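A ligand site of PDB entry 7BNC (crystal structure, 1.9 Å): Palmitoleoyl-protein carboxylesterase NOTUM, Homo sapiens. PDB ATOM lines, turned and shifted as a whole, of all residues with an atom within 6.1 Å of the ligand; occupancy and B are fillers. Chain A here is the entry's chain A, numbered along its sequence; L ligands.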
ATOM      1  N   GLY A  49      19.120 -19.777  16.931  1.00  0.00           N
ATOM      2  CA  GLY A  49      19.861 -20.846  16.316  1.00  0.00           C
ATOM      3  C   GLY A  49      20.815 -21.501  17.316  1.00  0.00           C
ATOM      4  O   GLY A  49      20.725 -21.272  18.520  1.00  0.00           O
ATOM      5  N   GLY A  50      21.747 -22.286  16.783  1.00  0.00           N
ATOM      6  CA  GLY A  50      22.766 -22.962  17.578  1.00  0.00           C
ATOM      7  C   GLY A  50      22.989 -24.436  17.284  1.00  0.00           C
ATOM      8  O   GLY A  50      22.976 -25.268  18.199  1.00  0.00           O
ATOM      9  N   TRP A  51      23.151 -24.787  16.003  1.00  0.00           N
ATOM     10  CA  TRP A  51      23.494 -26.152  15.564  1.00  0.00           C
ATOM     11  C   TRP A  51      22.385 -27.116  15.994  1.00  0.00           C
ATOM     12  O   TRP A  51      21.193 -26.771  15.872  1.00  0.00           O
ATOM     13  CB  TRP A  51      24.900 -26.507  16.029  1.00  0.00           C
ATOM     14  CG  TRP A  51      25.968 -25.703  15.295  1.00  0.00           C
ATOM     15  CD1 TRP A  51      26.497 -24.518  15.709  1.00  0.00           C
ATOM     16  CD2 TRP A  51      26.619 -26.014  14.053  1.00  0.00           C
ATOM     17  NE1 TRP A  51      27.455 -24.084  14.814  1.00  0.00           N
ATOM     18  CE2 TRP A  51      27.525 -24.968  13.773  1.00  0.00           C
ATOM     19  CE3 TRP A  51      26.524 -27.068  13.152  1.00  0.00           C
ATOM     20  CZ2 TRP A  51      28.350 -24.950  12.645  1.00  0.00           C
ATOM     21  CZ3 TRP A  51      27.355 -27.057  12.027  1.00  0.00           C
ATOM     22  CH2 TRP A  51      28.259 -26.000  11.797  1.00  0.00           C
ATOM     23  N   TYR A  52      22.724 -28.339  16.422  1.00  0.00           N
ATOM     24  CA  TYR A  52      21.798 -29.460  16.626  1.00  0.00           C
ATOM     25  C   TYR A  52      22.641 -30.593  17.187  1.00  0.00           C
ATOM     26  O   TYR A  52      23.865 -30.532  17.181  1.00  0.00           O
ATOM     27  CB  TYR A  52      21.116 -29.894  15.301  1.00  0.00           C
ATOM     28  CG  TYR A  52      22.133 -29.999  14.182  1.00  0.00           C
ATOM     29  CD1 TYR A  52      22.987 -31.095  14.083  1.00  0.00           C
ATOM     30  CD2 TYR A  52      22.274 -28.988  13.238  1.00  0.00           C
ATOM     31  CE1 TYR A  52      23.969 -31.169  13.056  1.00  0.00           C
ATOM     32  CE2 TYR A  52      23.239 -29.063  12.210  1.00  0.00           C
ATOM     33  CZ  TYR A  52      24.080 -30.147  12.128  1.00  0.00           C
ATOM     34  OH  TYR A  52      25.026 -30.210  11.101  1.00  0.00           O
ATOM     35  N   TYR A 105      16.043 -21.510  21.548  1.00  0.00           N
ATOM     36  CA  TYR A 105      16.203 -22.790  20.876  1.00  0.00           C
ATOM     37  C   TYR A 105      16.662 -23.784  21.925  1.00  0.00           C
ATOM     38  O   TYR A 105      17.825 -23.726  22.347  1.00  0.00           O
ATOM     39  CB  TYR A 105      17.230 -22.646  19.763  1.00  0.00           C
ATOM     40  CG  TYR A 105      17.589 -23.860  18.947  1.00  0.00           C
ATOM     41  CD1 TYR A 105      16.621 -24.750  18.480  1.00  0.00           C
ATOM     42  CD2 TYR A 105      18.918 -24.059  18.555  1.00  0.00           C
ATOM     43  CE1 TYR A 105      16.986 -25.852  17.698  1.00  0.00           C
ATOM     44  CE2 TYR A 105      19.278 -25.105  17.776  1.00  0.00           C
ATOM     45  CZ  TYR A 105      18.321 -26.004  17.354  1.00  0.00           C
ATOM     46  OH  TYR A 105      18.744 -27.042  16.560  1.00  0.00           O
ATOM     47  N   VAL A 110      16.762 -28.386  14.872  1.00  0.00           N
ATOM     48  CA  VAL A 110      16.581 -27.432  13.783  1.00  0.00           C
ATOM     49  C   VAL A 110      15.075 -27.098  13.754  1.00  0.00           C
ATOM     50  O   VAL A 110      14.491 -26.821  12.693  1.00  0.00           O
ATOM     51  CB  VAL A 110      17.089 -27.970  12.427  1.00  0.00           C
ATOM     52  CG1 VAL A 110      17.106 -26.846  11.334  1.00  0.00           C
ATOM     53  CG2 VAL A 110      18.449 -28.768  12.542  1.00  0.00           C
ATOM     54  N   SER A 154      17.602 -17.139  12.855  1.00  0.00           N
ATOM     55  CA  SER A 154      18.989 -17.101  12.416  1.00  0.00           C
ATOM     56  C   SER A 154      19.628 -18.479  12.554  1.00  0.00           C
ATOM     57  O   SER A 154      19.408 -19.167  13.550  1.00  0.00           O
ATOM     58  CB  SER A 154      19.811 -16.096  13.242  1.00  0.00           C
ATOM     59  OG  SER A 154      19.401 -14.770  12.964  1.00  0.00           O
ATOM     60  N   SER A 155      20.415 -18.865  11.537  1.00  0.00           N
ATOM     61  CA  SER A 155      21.201 -20.110  11.527  1.00  0.00           C
ATOM     62  C   SER A 155      20.231 -21.275  11.592  1.00  0.00           C
ATOM     63  O   SER A 155      19.377 -21.367  10.704  1.00  0.00           O
ATOM     64  CB  SER A 155      22.245 -20.116  12.640  1.00  0.00           C
ATOM     65  OG  SER A 155      23.105 -19.038  12.444  1.00  0.00           O
ATOM     66  N   ALA A 156      20.341 -22.193  12.572  1.00  0.00           N
ATOM     67  CA  ALA A 156      19.342 -23.265  12.692  1.00  0.00           C
ATOM     68  C   ALA A 156      17.942 -22.687  12.789  1.00  0.00           C
ATOM     69  O   ALA A 156      16.966 -23.348  12.401  1.00  0.00           O
ATOM     70  CB  ALA A 156      19.629 -24.147  13.919  1.00  0.00           C
ATOM     71  N   GLY A 157      17.814 -21.472  13.339  1.00  0.00           N
ATOM     72  CA  GLY A 157      16.503 -20.855  13.407  1.00  0.00           C
ATOM     73  C   GLY A 157      16.046 -20.331  12.064  1.00  0.00           C
ATOM     74  O   GLY A 157      14.841 -20.242  11.820  1.00  0.00           O
ATOM     75  N   THR A 159      16.802 -21.960   9.143  1.00  0.00           N
ATOM     76  CA  THR A 159      16.245 -23.171   8.567  1.00  0.00           C
ATOM     77  C   THR A 159      14.882 -23.500   9.218  1.00  0.00           C
ATOM     78  O   THR A 159      13.959 -23.928   8.541  1.00  0.00           O
ATOM     79  CB  THR A 159      17.212 -24.352   8.712  1.00  0.00           C
ATOM     80  OG1 THR A 159      18.506 -23.952   8.259  1.00  0.00           O
ATOM     81  CG2 THR A 159      16.763 -25.597   7.886  1.00  0.00           C
ATOM     82  N   SER A 188      20.617 -16.751   7.369  1.00  0.00           N
ATOM     83  CA  SER A 188      21.750 -17.667   7.524  1.00  0.00           C
ATOM     84  C   SER A 188      21.328 -19.121   7.710  1.00  0.00           C
ATOM     85  O   SER A 188      22.005 -19.901   8.390  1.00  0.00           O
ATOM     86  CB  SER A 188      22.622 -17.255   8.724  1.00  0.00           C
ATOM     87  OG  SER A 188      23.202 -15.983   8.502  1.00  0.00           O
ATOM     88  N   GLY A 189      20.226 -19.521   7.094  1.00  0.00           N
ATOM     89  CA  GLY A 189      19.821 -20.898   7.229  1.00  0.00           C
ATOM     90  C   GLY A 189      19.609 -21.553   5.878  1.00  0.00           C
ATOM     91  O   GLY A 189      18.860 -22.520   5.785  1.00  0.00           O
ATOM     92  N   PHE A 191      21.452 -23.457   3.336  1.00  0.00           N
ATOM     93  CA  PHE A 191      22.650 -24.266   3.194  1.00  0.00           C
ATOM     94  C   PHE A 191      22.643 -25.075   1.908  1.00  0.00           C
ATOM     95  O   PHE A 191      21.597 -25.337   1.316  1.00  0.00           O
ATOM     96  CB  PHE A 191      22.800 -25.223   4.385  1.00  0.00           C
ATOM     97  CG  PHE A 191      23.026 -24.527   5.678  1.00  0.00           C
ATOM     98  CD1 PHE A 191      24.297 -24.082   6.025  1.00  0.00           C
ATOM     99  CD2 PHE A 191      21.974 -24.301   6.564  1.00  0.00           C
ATOM    100  CE1 PHE A 191      24.499 -23.411   7.234  1.00  0.00           C
ATOM    101  CE2 PHE A 191      22.176 -23.637   7.784  1.00  0.00           C
ATOM    102  CZ  PHE A 191      23.401 -23.188   8.111  1.00  0.00           C
ATOM    103  N   LEU A 192      23.839 -25.509   1.508  1.00  0.00           N
ATOM    104  CA  LEU A 192      24.069 -26.331   0.331  1.00  0.00           C
ATOM    105  C   LEU A 192      24.527 -27.708   0.785  1.00  0.00           C
ATOM    106  O   LEU A 192      25.371 -27.817   1.674  1.00  0.00           O
ATOM    107  CB  LEU A 192      25.119 -25.715  -0.581  1.00  0.00           C
ATOM    108  CG  LEU A 192      24.799 -24.310  -1.118  1.00  0.00           C
ATOM    109  CD1 LEU A 192      25.929 -23.850  -2.020  1.00  0.00           C
ATOM    110  CD2 LEU A 192      23.422 -24.248  -1.817  1.00  0.00           C
ATOM    111  N   PRO A 210      27.294 -31.861   5.563  1.00  0.00           N
ATOM    112  CA  PRO A 210      25.921 -31.344   5.746  1.00  0.00           C
ATOM    113  C   PRO A 210      24.847 -32.388   5.478  1.00  0.00           C
ATOM    114  O   PRO A 210      23.917 -32.556   6.271  1.00  0.00           O
ATOM    115  CB  PRO A 210      25.853 -30.152   4.763  1.00  0.00           C
ATOM    116  CG  PRO A 210      27.057 -30.269   3.867  1.00  0.00           C
ATOM    117  CD  PRO A 210      28.094 -31.007   4.653  1.00  0.00           C
ATOM    118  N   THR A 211      24.995 -33.162   4.398  1.00  0.00           N
ATOM    119  CA  THR A 211      23.980 -34.135   4.022  1.00  0.00           C
ATOM    120  C   THR A 211      23.769 -35.178   5.110  1.00  0.00           C
ATOM    121  O   THR A 211      22.647 -35.377   5.582  1.00  0.00           O
ATOM    122  CB  THR A 211      24.369 -34.774   2.714  1.00  0.00           C
ATOM    123  OG1 THR A 211      24.170 -33.818   1.662  1.00  0.00           O
ATOM    124  CG2 THR A 211      23.555 -35.978   2.462  1.00  0.00           C
ATOM    125  N   ILE A 214      21.976 -34.359   8.700  1.00  0.00           N
ATOM    126  CA  ILE A 214      20.523 -34.226   8.755  1.00  0.00           C
ATOM    127  C   ILE A 214      19.819 -35.584   8.624  1.00  0.00           C
ATOM    128  O   ILE A 214      18.808 -35.829   9.283  1.00  0.00           O
ATOM    129  CB  ILE A 214      20.060 -33.237   7.676  1.00  0.00           C
ATOM    130  CG1 ILE A 214      20.812 -31.909   7.801  1.00  0.00           C
ATOM    131  CG2 ILE A 214      18.548 -33.054   7.758  1.00  0.00           C
ATOM    132  CD1 ILE A 214      20.695 -31.274   9.170  1.00  0.00           C
ATOM    133  N   PHE A 242      15.416 -29.901   4.524  1.00  0.00           N
ATOM    134  CA  PHE A 242      16.211 -29.045   5.396  1.00  0.00           C
ATOM    135  C   PHE A 242      17.116 -28.111   4.612  1.00  0.00           C
ATOM    136  O   PHE A 242      17.806 -27.311   5.236  1.00  0.00           O
ATOM    137  CB  PHE A 242      17.077 -29.857   6.371  1.00  0.00           C
ATOM    138  CG  PHE A 242      16.333 -30.396   7.518  1.00  0.00           C
ATOM    139  CD1 PHE A 242      15.295 -31.298   7.311  1.00  0.00           C
ATOM    140  CD2 PHE A 242      16.647 -29.998   8.818  1.00  0.00           C
ATOM    141  CE1 PHE A 242      14.566 -31.793   8.376  1.00  0.00           C
ATOM    142  CE2 PHE A 242      15.933 -30.470   9.873  1.00  0.00           C
ATOM    143  CZ  PHE A 242      14.875 -31.387   9.649  1.00  0.00           C
ATOM    144  N   PHE A 243      17.103 -28.198   3.279  1.00  0.00           N
ATOM    145  CA  PHE A 243      17.984 -27.417   2.418  1.00  0.00           C
ATOM    146  C   PHE A 243      17.156 -26.390   1.665  1.00  0.00           C
ATOM    147  O   PHE A 243      16.322 -26.747   0.827  1.00  0.00           O
ATOM    148  CB  PHE A 243      18.753 -28.338   1.483  1.00  0.00           C
ATOM    149  CG  PHE A 243      19.819 -29.068   2.205  1.00  0.00           C
ATOM    150  CD1 PHE A 243      19.550 -30.287   2.800  1.00  0.00           C
ATOM    151  CD2 PHE A 243      21.055 -28.475   2.424  1.00  0.00           C
ATOM    152  CE1 PHE A 243      20.503 -30.929   3.527  1.00  0.00           C
ATOM    153  CE2 PHE A 243      22.020 -29.124   3.171  1.00  0.00           C
ATOM    154  CZ  PHE A 243      21.739 -30.334   3.721  1.00  0.00           C
ATOM    155  N   ALA A 265      29.210 -21.156   8.921  1.00  0.00           N
ATOM    156  CA  ALA A 265      28.767 -22.496   9.271  1.00  0.00           C
ATOM    157  C   ALA A 265      28.830 -23.433   8.066  1.00  0.00           C
ATOM    158  O   ALA A 265      29.221 -24.593   8.193  1.00  0.00           O
ATOM    159  CB  ALA A 265      27.350 -22.441   9.852  1.00  0.00           C
ATOM    160  N   GLN A 266      28.463 -22.926   6.888  1.00  0.00           N
ATOM    161  CA  GLN A 266      28.667 -23.704   5.648  1.00  0.00           C
ATOM    162  C   GLN A 266      30.137 -24.081   5.445  1.00  0.00           C
ATOM    163  O   GLN A 266      30.467 -25.221   5.117  1.00  0.00           O
ATOM    164  CB  GLN A 266      28.154 -22.883   4.458  1.00  0.00           C
ATOM    165  CG  GLN A 266      28.274 -23.545   3.087  1.00  0.00           C
ATOM    166  CD  GLN A 266      27.201 -24.557   2.875  1.00  0.00           C
ATOM    167  OE1 GLN A 266      25.991 -24.248   2.909  1.00  0.00           O
ATOM    168  NE2 GLN A 266      27.621 -25.797   2.586  1.00  0.00           N
ATOM    169  N   VAL A 269      31.194 -26.917   7.918  1.00  0.00           N
ATOM    170  CA  VAL A 269      30.808 -28.260   7.536  1.00  0.00           C
ATOM    171  C   VAL A 269      31.465 -28.682   6.244  1.00  0.00           C
ATOM    172  O   VAL A 269      31.509 -29.875   5.961  1.00  0.00           O
ATOM    173  CB  VAL A 269      29.275 -28.400   7.416  1.00  0.00           C
ATOM    174  CG1 VAL A 269      28.635 -28.026   8.700  1.00  0.00           C
ATOM    175  CG2 VAL A 269      28.751 -27.550   6.298  1.00  0.00           C
ATOM    176  N   HIS A 312      28.448 -14.938   9.838  1.00  0.00           N
ATOM    177  CA  HIS A 312      27.420 -15.855  10.322  1.00  0.00           C
ATOM    178  C   HIS A 312      26.361 -15.065  11.088  1.00  0.00           C
ATOM    179  O   HIS A 312      26.699 -14.435  12.091  1.00  0.00           O
ATOM    180  CB  HIS A 312      28.045 -16.907  11.222  1.00  0.00           C
ATOM    181  CG  HIS A 312      27.114 -18.019  11.586  1.00  0.00           C
ATOM    182  ND1 HIS A 312      26.393 -18.727  10.641  1.00  0.00           N
ATOM    183  CD2 HIS A 312      26.786 -18.548  12.790  1.00  0.00           C
ATOM    184  CE1 HIS A 312      25.664 -19.645  11.256  1.00  0.00           C
ATOM    185  NE2 HIS A 312      25.894 -19.562  12.560  1.00  0.00           N
ATOM    186  N   GLU A 313      25.101 -15.130  10.630  1.00  0.00           N
ATOM    187  CA  GLU A 313      23.962 -14.442  11.234  1.00  0.00           C
ATOM    188  C   GLU A 313      24.031 -12.932  11.060  1.00  0.00           C
ATOM    189  O   GLU A 313      25.115 -12.370  10.914  1.00  0.00           O
ATOM    190  CB  GLU A 313      23.819 -14.739  12.733  1.00  0.00           C
ATOM    191  CG  GLU A 313      23.837 -16.206  13.027  1.00  0.00           C
ATOM    192  CD  GLU A 313      23.348 -16.511  14.434  1.00  0.00           C
ATOM    193  OE1 GLU A 313      23.312 -15.578  15.258  1.00  0.00           O
ATOM    194  OE2 GLU A 313      22.992 -17.666  14.725  1.00  0.00           O
HETATM  195  C1  LIG L   1      24.412 -23.552  12.541  1.00  0.00           C
HETATM  196  C2  LIG L   1      24.292 -27.114   8.353  1.00  0.00           C
HETATM  197  C3  LIG L   1      25.296 -26.517   9.065  1.00  0.00           C
HETATM  198  C4  LIG L   1      22.877 -26.933   8.780  1.00  0.00           C
HETATM  199  C5  LIG L   1      24.222 -28.035   7.029  1.00  0.00           C
HETATM  200  C6  LIG L   1      22.832 -28.309   6.820  1.00  0.00           C
HETATM  201  C7  LIG L   1      22.121 -27.648   7.883  1.00  0.00           C
HETATM  202  C8  LIG L   1      20.716 -27.626   8.056  1.00  0.00           C
HETATM  203  C9  LIG L   1      20.229 -26.889   9.170  1.00  0.00           C
HETATM  204  C10 LIG L   1      21.049 -26.174  10.064  1.00  0.00           C
HETATM  205  C11 LIG L   1      22.461 -26.247   9.813  1.00  0.00           C
HETATM  206  C12 LIG L   1      23.470 -25.605  10.598  1.00  0.00           C
HETATM  207  C13 LIG L   1      24.879 -25.740  10.211  1.00  0.00           C
HETATM  208  C14 LIG L   1      23.977 -22.589  13.652  1.00  0.00           C
HETATM  209  O1  LIG L   1      22.843 -22.743  14.172  1.00  0.00           O
HETATM  210  O2  LIG L   1      24.745 -21.651  14.067  1.00  0.00           O
HETATM  211  S1  LIG L   1      23.009 -24.625  12.029  1.00  0.00           S
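The backbone carbonyl oxygen (O) of Trp 51 lies within hydrogen-bond range of the side-chain hydroxyl (OH) of Tyr 105. NE2 of His 312 is in hydrogen-bond range of OG of Ser 155, 2.8 Å away. The side-chain carboxylate of Glu 313 is in hydrogen-bond range of the side-chain hydroxyl of Ser 155. O of Gly 189 lies within hydrogen-bond range of OG1 of Thr 159, at 2.9 Å. The backbone NH (N) of Val 110 lies within hydrogen-bond range of the side-chain hydroxyl (OH) of Tyr 105 (2.9 Å). The backbone NH (N) of Gly 49 lies close to the backbone carbonyl oxygen (O) of Ser 154.
N of Trp 51 is in hydrogen-bond range of O1 of the ligand (2.8 Å). An oxygen (O2) of the ligand sits at hydrogen-bond distance from a ring nitrogen (NE2) of His 312 (2.8 Å). The backbone NH of Gly 50 sits at hydrogen-bond distance from an oxygen (O1) of the ligand (2.9 Å). The backbone NH (N) of Ala 156 lies within hydrogen-bond range of an oxygen (O1) of the ligand. The side-chain hydroxyl (OG) of Ser 155 sits close to an oxygen (O2) of the ligand (3.5 Å).
Gly 49 touches the ligand. Tyr 52 touches the ligand (CE2 to C11, 3.8 Å). Val 110 touches the ligand (CG1 to C9, 3.8 Å). Thr 159 touches the ligand. CE2 of Phe 191 touches C11 of the ligand (3.3 Å). CB of Pro 210 touches C5 of the ligand, 3.5 Å away. Ile 214 touches the ligand. Phe 243 touches the ligand. Val 269 touches the ligand. Hydrophobic or aromatic side chains that line the ligand: Trp 51, Tyr 52, Val 110, Ala 156, Phe 191, Pro 210, Ile 214, Phe 243, Val 269 and His 312. 14 residues have an atom within 4 Å of the ligand: Gly 49, Gly 50, Trp 51, Tyr 52, Val 110, Ser 155, Ala 156, Thr 159, Phe 191, Pro 210, Ile 214, Phe 243, Val 269 and His 312. Along chain A the residues within 4 Å of the ligand span positions 49 to 312. The nearest printed residue that does not touch the ligand is Phe 242 (4.1 Å).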
